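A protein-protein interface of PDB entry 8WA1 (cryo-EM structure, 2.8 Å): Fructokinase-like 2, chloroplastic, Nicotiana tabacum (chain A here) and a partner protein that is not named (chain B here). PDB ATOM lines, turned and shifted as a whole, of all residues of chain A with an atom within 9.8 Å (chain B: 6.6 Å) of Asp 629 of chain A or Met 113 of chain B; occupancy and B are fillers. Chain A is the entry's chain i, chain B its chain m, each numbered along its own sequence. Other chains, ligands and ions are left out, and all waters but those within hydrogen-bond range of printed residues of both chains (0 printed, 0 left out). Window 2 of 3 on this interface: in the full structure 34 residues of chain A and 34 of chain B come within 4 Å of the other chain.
The side-chain amide nitrogen (NE2) of Gln 109 of chain B lies within hydrogen-bond range of the side-chain hydroxyl (OH) of Tyr 560 of chain A (3.2 Å). The side-chain amide oxygen of Gln 109 of chain B sits close to the side-chain carboxylate of Asp 630 of chain A. The side-chain amide oxygen (OE1) of Gln 109 of chain B lies within hydrogen-bond range of the backbone NH (N) of His 631 of chain A, at 3.2 Å. The side-chain sulfur of Met 113 of chain B is in hydrogen-bond range of the backbone NH of Asp 629 of chain A, at 3.4 Å. The side-chain carboxylate (OE1) of Glu 110 of chain B lies close to the side-chain carboxylate (OD1) of Asp 629 of chain A.
Hydrophobic or aromatic side chains of chain B within 4 Å of the printed part of chain A: Leu 106, Met 113 and Ile 167. Of the 11 printed residues of chain A, 4 touch a printed residue of chain B. Printed residues of chain A that touch a printed residue of chain B: Tyr 560, Asp 629, Asp 630 and His 631. Among the printed residues, 9 pairs touch across the chains.
Printed residues of chain B within 4 Å of Tyr 560 of chain A: Leu 106 (3.6 Å) and Gln 109 (3.2 Å). Of chain B, only Gln 109, Glu 110, Met 113 and Ile 167 come within 4 Å of Asp 629 of chain A. Of the printed residues of chain B, His 631 of chain A touches Gln 109. Of the printed residues of chain A, Leu 106 of chain B touches Tyr 560 and Asp 630. Of the printed residues of chain A, Gln 109 of chain B touches Tyr 560, Asp 629, Asp 630 and His 631. Of the printed residues of chain A, Glu 110 of chain B touches Asp 629. No residue of chain A comes within 4 Å of Glu 112 of chain B. No residue of chain A comes within 4 Å of Val 116 of chain B.
Among the printed residues, merely in contact across the chains: Tyr 560 of chain A with Leu 106 of chain B, Asp 629 of chain A with Gln 109 of chain B, Asp 629 of chain A with Ile 167 of chain B and Asp 630 of chain A with Leu 106 of chain B.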
ATOM      1  N   HIS A 288      20.666   4.516  36.054  1.00  0.00           N
ATOM      2  CA  HIS A 288      19.295   4.130  36.353  1.00  0.00           C
ATOM      3  C   HIS A 288      18.724   3.319  35.198  1.00  0.00           C
ATOM      4  O   HIS A 288      18.602   3.829  34.079  1.00  0.00           O
ATOM      5  CB  HIS A 288      18.428   5.366  36.612  1.00  0.00           C
ATOM      6  CG  HIS A 288      17.001   5.046  36.927  1.00  0.00           C
ATOM      7  ND1 HIS A 288      16.628   4.325  38.041  1.00  0.00           N
ATOM      8  CD2 HIS A 288      15.855   5.347  36.272  1.00  0.00           C
ATOM      9  CE1 HIS A 288      15.312   4.198  38.059  1.00  0.00           C
ATOM     10  NE2 HIS A 288      14.821   4.808  36.997  1.00  0.00           N
ATOM     11  N   TYR A 560       8.522  -5.210  31.925  1.00  0.00           N
ATOM     12  CA  TYR A 560       9.649  -4.483  32.498  1.00  0.00           C
ATOM     13  C   TYR A 560      10.661  -5.428  33.138  1.00  0.00           C
ATOM     14  O   TYR A 560      11.865  -5.197  33.055  1.00  0.00           O
ATOM     15  CB  TYR A 560       9.165  -3.460  33.524  1.00  0.00           C
ATOM     16  CG  TYR A 560       8.097  -2.520  33.008  1.00  0.00           C
ATOM     17  CD1 TYR A 560       8.169  -1.983  31.730  1.00  0.00           C
ATOM     18  CD2 TYR A 560       7.025  -2.158  33.810  1.00  0.00           C
ATOM     19  CE1 TYR A 560       7.195  -1.125  31.261  1.00  0.00           C
ATOM     20  CE2 TYR A 560       6.047  -1.297  33.352  1.00  0.00           C
ATOM     21  CZ  TYR A 560       6.139  -0.782  32.078  1.00  0.00           C
ATOM     22  OH  TYR A 560       5.168   0.077  31.619  1.00  0.00           O
ATOM     23  N   PRO A 618      -0.111  -0.945  30.694  1.00  0.00           N
ATOM     24  CA  PRO A 618      -1.561  -1.003  30.490  1.00  0.00           C
ATOM     25  C   PRO A 618      -1.914  -1.841  29.273  1.00  0.00           C
ATOM     26  O   PRO A 618      -1.173  -1.900  28.289  1.00  0.00           O
ATOM     27  CB  PRO A 618      -1.949   0.466  30.288  1.00  0.00           C
ATOM     28  CG  PRO A 618      -0.709   1.106  29.765  1.00  0.00           C
ATOM     29  CD  PRO A 618       0.428   0.403  30.451  1.00  0.00           C
ATOM     30  N   ASP A 625      -4.881   6.801  35.201  1.00  0.00           N
ATOM     31  CA  ASP A 625      -4.166   8.034  35.502  1.00  0.00           C
ATOM     32  C   ASP A 625      -2.670   7.842  35.285  1.00  0.00           C
ATOM     33  O   ASP A 625      -2.080   6.857  35.738  1.00  0.00           O
ATOM     34  CB  ASP A 625      -4.442   8.469  36.942  1.00  0.00           C
ATOM     35  CG  ASP A 625      -3.624   9.678  37.355  1.00  0.00           C
ATOM     36  OD1 ASP A 625      -3.874  10.779  36.824  1.00  0.00           O
ATOM     37  OD2 ASP A 625      -2.730   9.526  38.215  1.00  0.00           O
ATOM     38  N   VAL A 626      -2.057   8.793  34.586  1.00  0.00           N
ATOM     39  CA  VAL A 626      -0.665   8.688  34.167  1.00  0.00           C
ATOM     40  C   VAL A 626       0.199   9.551  35.076  1.00  0.00           C
ATOM     41  O   VAL A 626      -0.183  10.672  35.435  1.00  0.00           O
ATOM     42  CB  VAL A 626      -0.498   9.096  32.691  1.00  0.00           C
ATOM     43  CG1 VAL A 626      -1.230   8.119  31.786  1.00  0.00           C
ATOM     44  CG2 VAL A 626      -1.011  10.509  32.458  1.00  0.00           C
ATOM     45  N   VAL A 627       1.347   9.015  35.476  1.00  0.00           N
ATOM     46  CA  VAL A 627       2.373   9.784  36.175  1.00  0.00           C
ATOM     47  C   VAL A 627       3.218  10.453  35.094  1.00  0.00           C
ATOM     48  O   VAL A 627       3.006  10.171  33.904  1.00  0.00           O
ATOM     49  CB  VAL A 627       3.206   8.889  37.108  1.00  0.00           C
ATOM     50  CG1 VAL A 627       2.296   8.066  38.011  1.00  0.00           C
ATOM     51  CG2 VAL A 627       4.138   7.992  36.309  1.00  0.00           C
ATOM     52  N   PRO A 628       4.154  11.362  35.433  1.00  0.00           N
ATOM     53  CA  PRO A 628       5.029  11.923  34.394  1.00  0.00           C
ATOM     54  C   PRO A 628       5.714  10.861  33.549  1.00  0.00           C
ATOM     55  O   PRO A 628       6.419   9.992  34.073  1.00  0.00           O
ATOM     56  CB  PRO A 628       6.043  12.739  35.202  1.00  0.00           C
ATOM     57  CG  PRO A 628       5.261  13.206  36.372  1.00  0.00           C
ATOM     58  CD  PRO A 628       4.311  12.081  36.713  1.00  0.00           C
ATOM     59  N   ASP A 629       5.456  10.903  32.242  1.00  0.00           N
ATOM     60  CA  ASP A 629       6.016  10.079  31.168  1.00  0.00           C
ATOM     61  C   ASP A 629       5.840   8.579  31.395  1.00  0.00           C
ATOM     62  O   ASP A 629       6.455   7.794  30.659  1.00  0.00           O
ATOM     63  CB  ASP A 629       7.504  10.376  30.890  1.00  0.00           C
ATOM     64  CG  ASP A 629       8.416  10.031  32.056  1.00  0.00           C
ATOM     65  OD1 ASP A 629       8.583   8.832  32.362  1.00  0.00           O
ATOM     66  OD2 ASP A 629       8.974  10.965  32.667  1.00  0.00           O
ATOM     67  N   ASP A 630       5.033   8.146  32.360  1.00  0.00           N
ATOM     68  CA  ASP A 630       4.866   6.722  32.617  1.00  0.00           C
ATOM     69  C   ASP A 630       3.439   6.437  33.058  1.00  0.00           C
ATOM     70  O   ASP A 630       2.739   7.319  33.561  1.00  0.00           O
ATOM     71  CB  ASP A 630       5.858   6.223  33.672  1.00  0.00           C
ATOM     72  CG  ASP A 630       7.241   5.975  33.101  1.00  0.00           C
ATOM     73  OD1 ASP A 630       7.333   5.402  31.993  1.00  0.00           O
ATOM     74  OD2 ASP A 630       8.235   6.351  33.756  1.00  0.00           O
ATOM     75  N   HIS A 631       3.014   5.194  32.840  1.00  0.00           N
ATOM     76  CA  HIS A 631       1.728   4.696  33.310  1.00  0.00           C
ATOM     77  C   HIS A 631       1.830   3.190  33.502  1.00  0.00           C
ATOM     78  O   HIS A 631       2.129   2.461  32.551  1.00  0.00           O
ATOM     79  CB  HIS A 631       0.602   5.050  32.331  1.00  0.00           C
ATOM     80  CG  HIS A 631       0.968   4.867  30.892  1.00  0.00           C
ATOM     81  ND1 HIS A 631       1.351   3.651  30.368  1.00  0.00           N
ATOM     82  CD2 HIS A 631       1.006   5.747  29.863  1.00  0.00           C
ATOM     83  CE1 HIS A 631       1.609   3.790  29.080  1.00  0.00           C
ATOM     84  NE2 HIS A 631       1.408   5.052  28.748  1.00  0.00           N
ATOM     85  N   GLY A 632       1.591   2.730  34.728  1.00  0.00           N
ATOM     86  CA  GLY A 632       1.680   1.318  35.042  1.00  0.00           C
ATOM     87  C   GLY A 632       0.563   0.832  35.944  1.00  0.00           C
ATOM     88  O   GLY A 632       0.111   1.564  36.828  1.00  0.00           O
ATOM     89  N   LEU B 106       9.795   1.149  28.842  1.00  0.00           N
ATOM     90  CA  LEU B 106       9.365   2.360  29.521  1.00  0.00           C
ATOM     91  C   LEU B 106       9.755   3.594  28.728  1.00  0.00           C
ATOM     92  O   LEU B 106       8.923   4.446  28.484  1.00  0.00           O
ATOM     93  CB  LEU B 106      10.021   2.427  30.882  1.00  0.00           C
ATOM     94  CG  LEU B 106       9.617   1.418  31.949  1.00  0.00           C
ATOM     95  CD1 LEU B 106      10.808   1.007  32.795  1.00  0.00           C
ATOM     96  CD2 LEU B 106       8.516   1.998  32.817  1.00  0.00           C
ATOM     97  N   MET B 107      11.011   3.716  28.349  1.00  0.00           N
ATOM     98  CA  MET B 107      11.533   4.830  27.561  1.00  0.00           C
ATOM     99  C   MET B 107      10.630   5.158  26.377  1.00  0.00           C
ATOM    100  O   MET B 107      10.552   6.321  25.961  1.00  0.00           O
ATOM    101  CB  MET B 107      12.950   4.514  27.079  1.00  0.00           C
ATOM    102  CG  MET B 107      13.610   5.640  26.294  1.00  0.00           C
ATOM    103  SD  MET B 107      14.177   7.003  27.329  1.00  0.00           S
ATOM    104  CE  MET B 107      15.890   6.546  27.585  1.00  0.00           C
ATOM    105  N   ALA B 108       9.953   4.153  25.819  1.00  0.00           N
ATOM    106  CA  ALA B 108       9.057   4.400  24.694  1.00  0.00           C
ATOM    107  C   ALA B 108       7.898   5.303  25.098  1.00  0.00           C
ATOM    108  O   ALA B 108       7.447   6.138  24.308  1.00  0.00           O
ATOM    109  CB  ALA B 108       8.537   3.076  24.134  1.00  0.00           C
ATOM    110  N   GLN B 109       7.408   5.156  26.331  1.00  0.00           N
ATOM    111  CA  GLN B 109       6.331   6.018  26.806  1.00  0.00           C
ATOM    112  C   GLN B 109       6.807   7.459  26.962  1.00  0.00           C
ATOM    113  O   GLN B 109       6.078   8.402  26.628  1.00  0.00           O
ATOM    114  CB  GLN B 109       5.778   5.481  28.126  1.00  0.00           C
ATOM    115  CG  GLN B 109       5.274   4.049  28.034  1.00  0.00           C
ATOM    116  CD  GLN B 109       4.833   3.495  29.372  1.00  0.00           C
ATOM    117  OE1 GLN B 109       4.826   4.202  30.379  1.00  0.00           O
ATOM    118  NE2 GLN B 109       4.461   2.219  29.390  1.00  0.00           N
ATOM    119  N   GLU B 110       8.029   7.646  27.467  1.00  0.00           N
ATOM    120  CA  GLU B 110       8.595   8.989  27.542  1.00  0.00           C
ATOM    121  C   GLU B 110       8.756   9.588  26.151  1.00  0.00           C
ATOM    122  O   GLU B 110       8.473  10.773  25.940  1.00  0.00           O
ATOM    123  CB  GLU B 110       9.941   8.959  28.262  1.00  0.00           C
ATOM    124  CG  GLU B 110       9.968   8.130  29.531  1.00  0.00           C
ATOM    125  CD  GLU B 110      11.271   8.285  30.288  1.00  0.00           C
ATOM    126  OE1 GLU B 110      11.268   8.107  31.524  1.00  0.00           O
ATOM    127  OE2 GLU B 110      12.296   8.594  29.646  1.00  0.00           O
ATOM    128  N   LEU B 111       9.209   8.780  25.190  1.00  0.00           N
ATOM    129  CA  LEU B 111       9.351   9.259  23.820  1.00  0.00           C
ATOM    130  C   LEU B 111       8.002   9.650  23.229  1.00  0.00           C
ATOM    131  O   LEU B 111       7.892  10.660  22.524  1.00  0.00           O
ATOM    132  CB  LEU B 111      10.023   8.193  22.957  1.00  0.00           C
ATOM    133  CG  LEU B 111      11.480   7.857  23.281  1.00  0.00           C
ATOM    134  CD1 LEU B 111      11.937   6.663  22.464  1.00  0.00           C
ATOM    135  CD2 LEU B 111      12.376   9.057  23.028  1.00  0.00           C
ATOM    136  N   GLU B 112       6.963   8.859  23.504  1.00  0.00           N
ATOM    137  CA  GLU B 112       5.631   9.184  23.005  1.00  0.00           C
ATOM    138  C   GLU B 112       5.117  10.481  23.616  1.00  0.00           C
ATOM    139  O   GLU B 112       4.556  11.329  22.911  1.00  0.00           O
ATOM    140  CB  GLU B 112       4.668   8.033  23.291  1.00  0.00           C
ATOM    141  CG  GLU B 112       3.905   7.537  22.070  1.00  0.00           C
ATOM    142  CD  GLU B 112       2.869   8.530  21.579  1.00  0.00           C
ATOM    143  OE1 GLU B 112       2.353   9.313  22.404  1.00  0.00           O
ATOM    144  OE2 GLU B 112       2.572   8.529  20.366  1.00  0.00           O
ATOM    145  N   MET B 113       5.305  10.658  24.927  1.00  0.00           N
ATOM    146  CA  MET B 113       4.869  11.899  25.560  1.00  0.00           C
ATOM    147  C   MET B 113       5.653  13.096  25.031  1.00  0.00           C
ATOM    148  O   MET B 113       5.096  14.188  24.874  1.00  0.00           O
ATOM    149  CB  MET B 113       5.002  11.802  27.079  1.00  0.00           C
ATOM    150  CG  MET B 113       4.458  13.021  27.810  1.00  0.00           C
ATOM    151  SD  MET B 113       4.587  12.924  29.603  1.00  0.00           S
ATOM    152  CE  MET B 113       3.845  14.484  30.077  1.00  0.00           C
ATOM    153  N   LEU B 114       6.941  12.907  24.740  1.00  0.00           N
ATOM    154  CA  LEU B 114       7.741  13.998  24.193  1.00  0.00           C
ATOM    155  C   LEU B 114       7.294  14.349  22.780  1.00  0.00           C
ATOM    156  O   LEU B 114       7.257  15.528  22.406  1.00  0.00           O
ATOM    157  CB  LEU B 114       9.222  13.623  24.211  1.00  0.00           C
ATOM    158  CG  LEU B 114      10.202  14.738  23.843  1.00  0.00           C
ATOM    159  CD1 LEU B 114      10.101  15.877  24.844  1.00  0.00           C
ATOM    160  CD2 LEU B 114      11.623  14.204  23.772  1.00  0.00           C
ATOM    161  N   ALA B 115       6.955  13.337  21.978  1.00  0.00           N
ATOM    162  CA  ALA B 115       6.432  13.595  20.641  1.00  0.00           C
ATOM    163  C   ALA B 115       5.077  14.286  20.707  1.00  0.00           C
ATOM    164  O   ALA B 115       4.731  15.081  19.827  1.00  0.00           O
ATOM    165  CB  ALA B 115       6.335  12.289  19.853  1.00  0.00           C
ATOM    166  N   VAL B 116       4.290  13.984  21.742  1.00  0.00           N
ATOM    167  CA  VAL B 116       3.031  14.698  21.945  1.00  0.00           C
ATOM    168  C   VAL B 116       3.299  16.155  22.301  1.00  0.00           C
ATOM    169  O   VAL B 116       2.642  17.067  21.787  1.00  0.00           O
ATOM    170  CB  VAL B 116       2.181  13.994  23.019  1.00  0.00           C
ATOM    171  CG1 VAL B 116       1.006  14.869  23.426  1.00  0.00           C
ATOM    172  CG2 VAL B 116       1.688  12.653  22.507  1.00  0.00           C
ATOM    173  N   GLU B 117       4.273  16.397  23.184  1.00  0.00           N
ATOM    174  CA  GLU B 117       4.595  17.767  23.572  1.00  0.00           C
ATOM    175  C   GLU B 117       5.200  18.546  22.411  1.00  0.00           C
ATOM    176  O   GLU B 117       4.976  19.754  22.281  1.00  0.00           O
ATOM    177  CB  GLU B 117       5.545  17.765  24.771  1.00  0.00           C
ATOM    178  CG  GLU B 117       4.942  17.191  26.046  1.00  0.00           C
ATOM    179  CD  GLU B 117       3.822  18.046  26.608  1.00  0.00           C
ATOM    180  OE1 GLU B 117       3.761  19.249  26.275  1.00  0.00           O
ATOM    181  OE2 GLU B 117       2.999  17.515  27.382  1.00  0.00           O
ATOM    182  N   TYR B 118       5.971  17.874  21.559  1.00  0.00           N
ATOM    183  CA  TYR B 118       6.585  18.483  20.378  1.00  0.00           C
ATOM    184  C   TYR B 118       6.051  17.749  19.153  1.00  0.00           C
ATOM    185  O   TYR B 118       6.646  16.776  18.685  1.00  0.00           O
ATOM    186  CB  TYR B 118       8.117  18.420  20.456  1.00  0.00           C
ATOM    187  CG  TYR B 118       8.714  19.200  21.606  1.00  0.00           C
ATOM    188  CD1 TYR B 118       8.829  18.635  22.870  1.00  0.00           C
ATOM    189  CD2 TYR B 118       9.165  20.501  21.428  1.00  0.00           C
ATOM    190  CE1 TYR B 118       9.373  19.345  23.924  1.00  0.00           C
ATOM    191  CE2 TYR B 118       9.712  21.219  22.476  1.00  0.00           C
ATOM    192  CZ  TYR B 118       9.813  20.635  23.721  1.00  0.00           C
ATOM    193  OH  TYR B 118      10.357  21.344  24.768  1.00  0.00           O
ATOM    194  N   ILE B 124      11.052  11.967  16.287  1.00  0.00           N
ATOM    195  CA  ILE B 124      11.478  10.873  17.154  1.00  0.00           C
ATOM    196  C   ILE B 124      11.332   9.571  16.378  1.00  0.00           C
ATOM    197  O   ILE B 124      10.223   9.208  15.969  1.00  0.00           O
ATOM    198  CB  ILE B 124      10.668  10.827  18.458  1.00  0.00           C
ATOM    199  CG1 ILE B 124      10.825  12.141  19.227  1.00  0.00           C
ATOM    200  CG2 ILE B 124      11.101   9.648  19.313  1.00  0.00           C
ATOM    201  CD1 ILE B 124      10.055  12.183  20.526  1.00  0.00           C
ATOM    202  N   ILE B 165      16.185   8.058  31.689  1.00  0.00           N
ATOM    203  CA  ILE B 165      16.383   9.448  32.093  1.00  0.00           C
ATOM    204  C   ILE B 165      15.034  10.145  32.230  1.00  0.00           C
ATOM    205  O   ILE B 165      14.064   9.755  31.566  1.00  0.00           O
ATOM    206  CB  ILE B 165      17.287  10.186  31.095  1.00  0.00           C
ATOM    207  CG1 ILE B 165      16.740  10.037  29.674  1.00  0.00           C
ATOM    208  CG2 ILE B 165      18.714   9.666  31.181  1.00  0.00           C
ATOM    209  CD1 ILE B 165      17.595  10.702  28.620  1.00  0.00           C
ATOM    210  N   PRO B 166      14.925  11.167  33.077  1.00  0.00           N
ATOM    211  CA  PRO B 166      13.654  11.886  33.207  1.00  0.00           C
ATOM    212  C   PRO B 166      13.307  12.652  31.939  1.00  0.00           C
ATOM    213  O   PRO B 166      14.166  12.995  31.123  1.00  0.00           O
ATOM    214  CB  PRO B 166      13.904  12.844  34.379  1.00  0.00           C
ATOM    215  CG  PRO B 166      15.072  12.265  35.112  1.00  0.00           C
ATOM    216  CD  PRO B 166      15.919  11.623  34.060  1.00  0.00           C
ATOM    217  N   ILE B 167      12.009  12.918  31.786  1.00  0.00           N
ATOM    218  CA  ILE B 167      11.531  13.634  30.606  1.00  0.00           C
ATOM    219  C   ILE B 167      11.958  15.096  30.658  1.00  0.00           C
ATOM    220  O   ILE B 167      12.165  15.736  29.619  1.00  0.00           O
ATOM    221  CB  ILE B 167      10.003  13.481  30.473  1.00  0.00           C
ATOM    222  CG1 ILE B 167       9.510  14.086  29.157  1.00  0.00           C
ATOM    223  CG2 ILE B 167       9.288  14.107  31.664  1.00  0.00           C
ATOM    224  CD1 ILE B 167       8.054  13.803  28.863  1.00  0.00           C
ATOM    225  N   GLN B 168      12.102  15.648  31.866  1.00  0.00           N
ATOM    226  CA  GLN B 168      12.502  17.045  31.993  1.00  0.00           C
ATOM    227  C   GLN B 168      13.918  17.262  31.475  1.00  0.00           C
ATOM    228  O   GLN B 168      14.209  18.288  30.848  1.00  0.00           O
ATOM    229  CB  GLN B 168      12.383  17.496  33.449  1.00  0.00           C
ATOM    230  CG  GLN B 168      12.752  18.954  33.681  1.00  0.00           C
ATOM    231  CD  GLN B 168      11.870  19.914  32.903  1.00  0.00           C
ATOM    232  OE1 GLN B 168      10.717  19.610  32.594  1.00  0.00           O
ATOM    233  NE2 GLN B 168      12.412  21.083  32.582  1.00  0.00           N
ATOM    234  N   MET B 170      15.341  15.482  29.089  1.00  0.00           N
ATOM    235  CA  MET B 170      15.240  15.412  27.636  1.00  0.00           C
ATOM    236  C   MET B 170      14.706  16.718  27.057  1.00  0.00           C
ATOM    237  O   MET B 170      15.188  17.191  26.020  1.00  0.00           O
ATOM    238  CB  MET B 170      14.350  14.241  27.224  1.00  0.00           C
ATOM    239  CG  MET B 170      14.785  12.900  27.790  1.00  0.00           C
ATOM    240  SD  MET B 170      13.881  11.513  27.078  1.00  0.00           S
ATOM    241  CE  MET B 170      12.191  11.973  27.452  1.00  0.00           C
ATOM    242  N   ARG B 171      13.706  17.311  27.715  1.00  0.00           N
ATOM    243  CA  ARG B 171      13.186  18.595  27.253  1.00  0.00           C
ATOM    244  C   ARG B 171      14.252  19.678  27.334  1.00  0.00           C
ATOM    245  O   ARG B 171      14.422  20.463  26.393  1.00  0.00           O
ATOM    246  CB  ARG B 171      11.951  18.991  28.065  1.00  0.00           C
ATOM    247  CG  ARG B 171      10.715  18.160  27.758  1.00  0.00           C
ATOM    248  CD  ARG B 171       9.453  18.821  28.293  1.00  0.00           C
ATOM    249  NE  ARG B 171       9.398  18.820  29.752  1.00  0.00           N
ATOM    250  CZ  ARG B 171       8.710  17.939  30.471  1.00  0.00           C
ATOM    251  NH1 ARG B 171       8.714  18.012  31.795  1.00  0.00           N
ATOM    252  NH2 ARG B 171       8.013  16.988  29.866  1.00  0.00           N
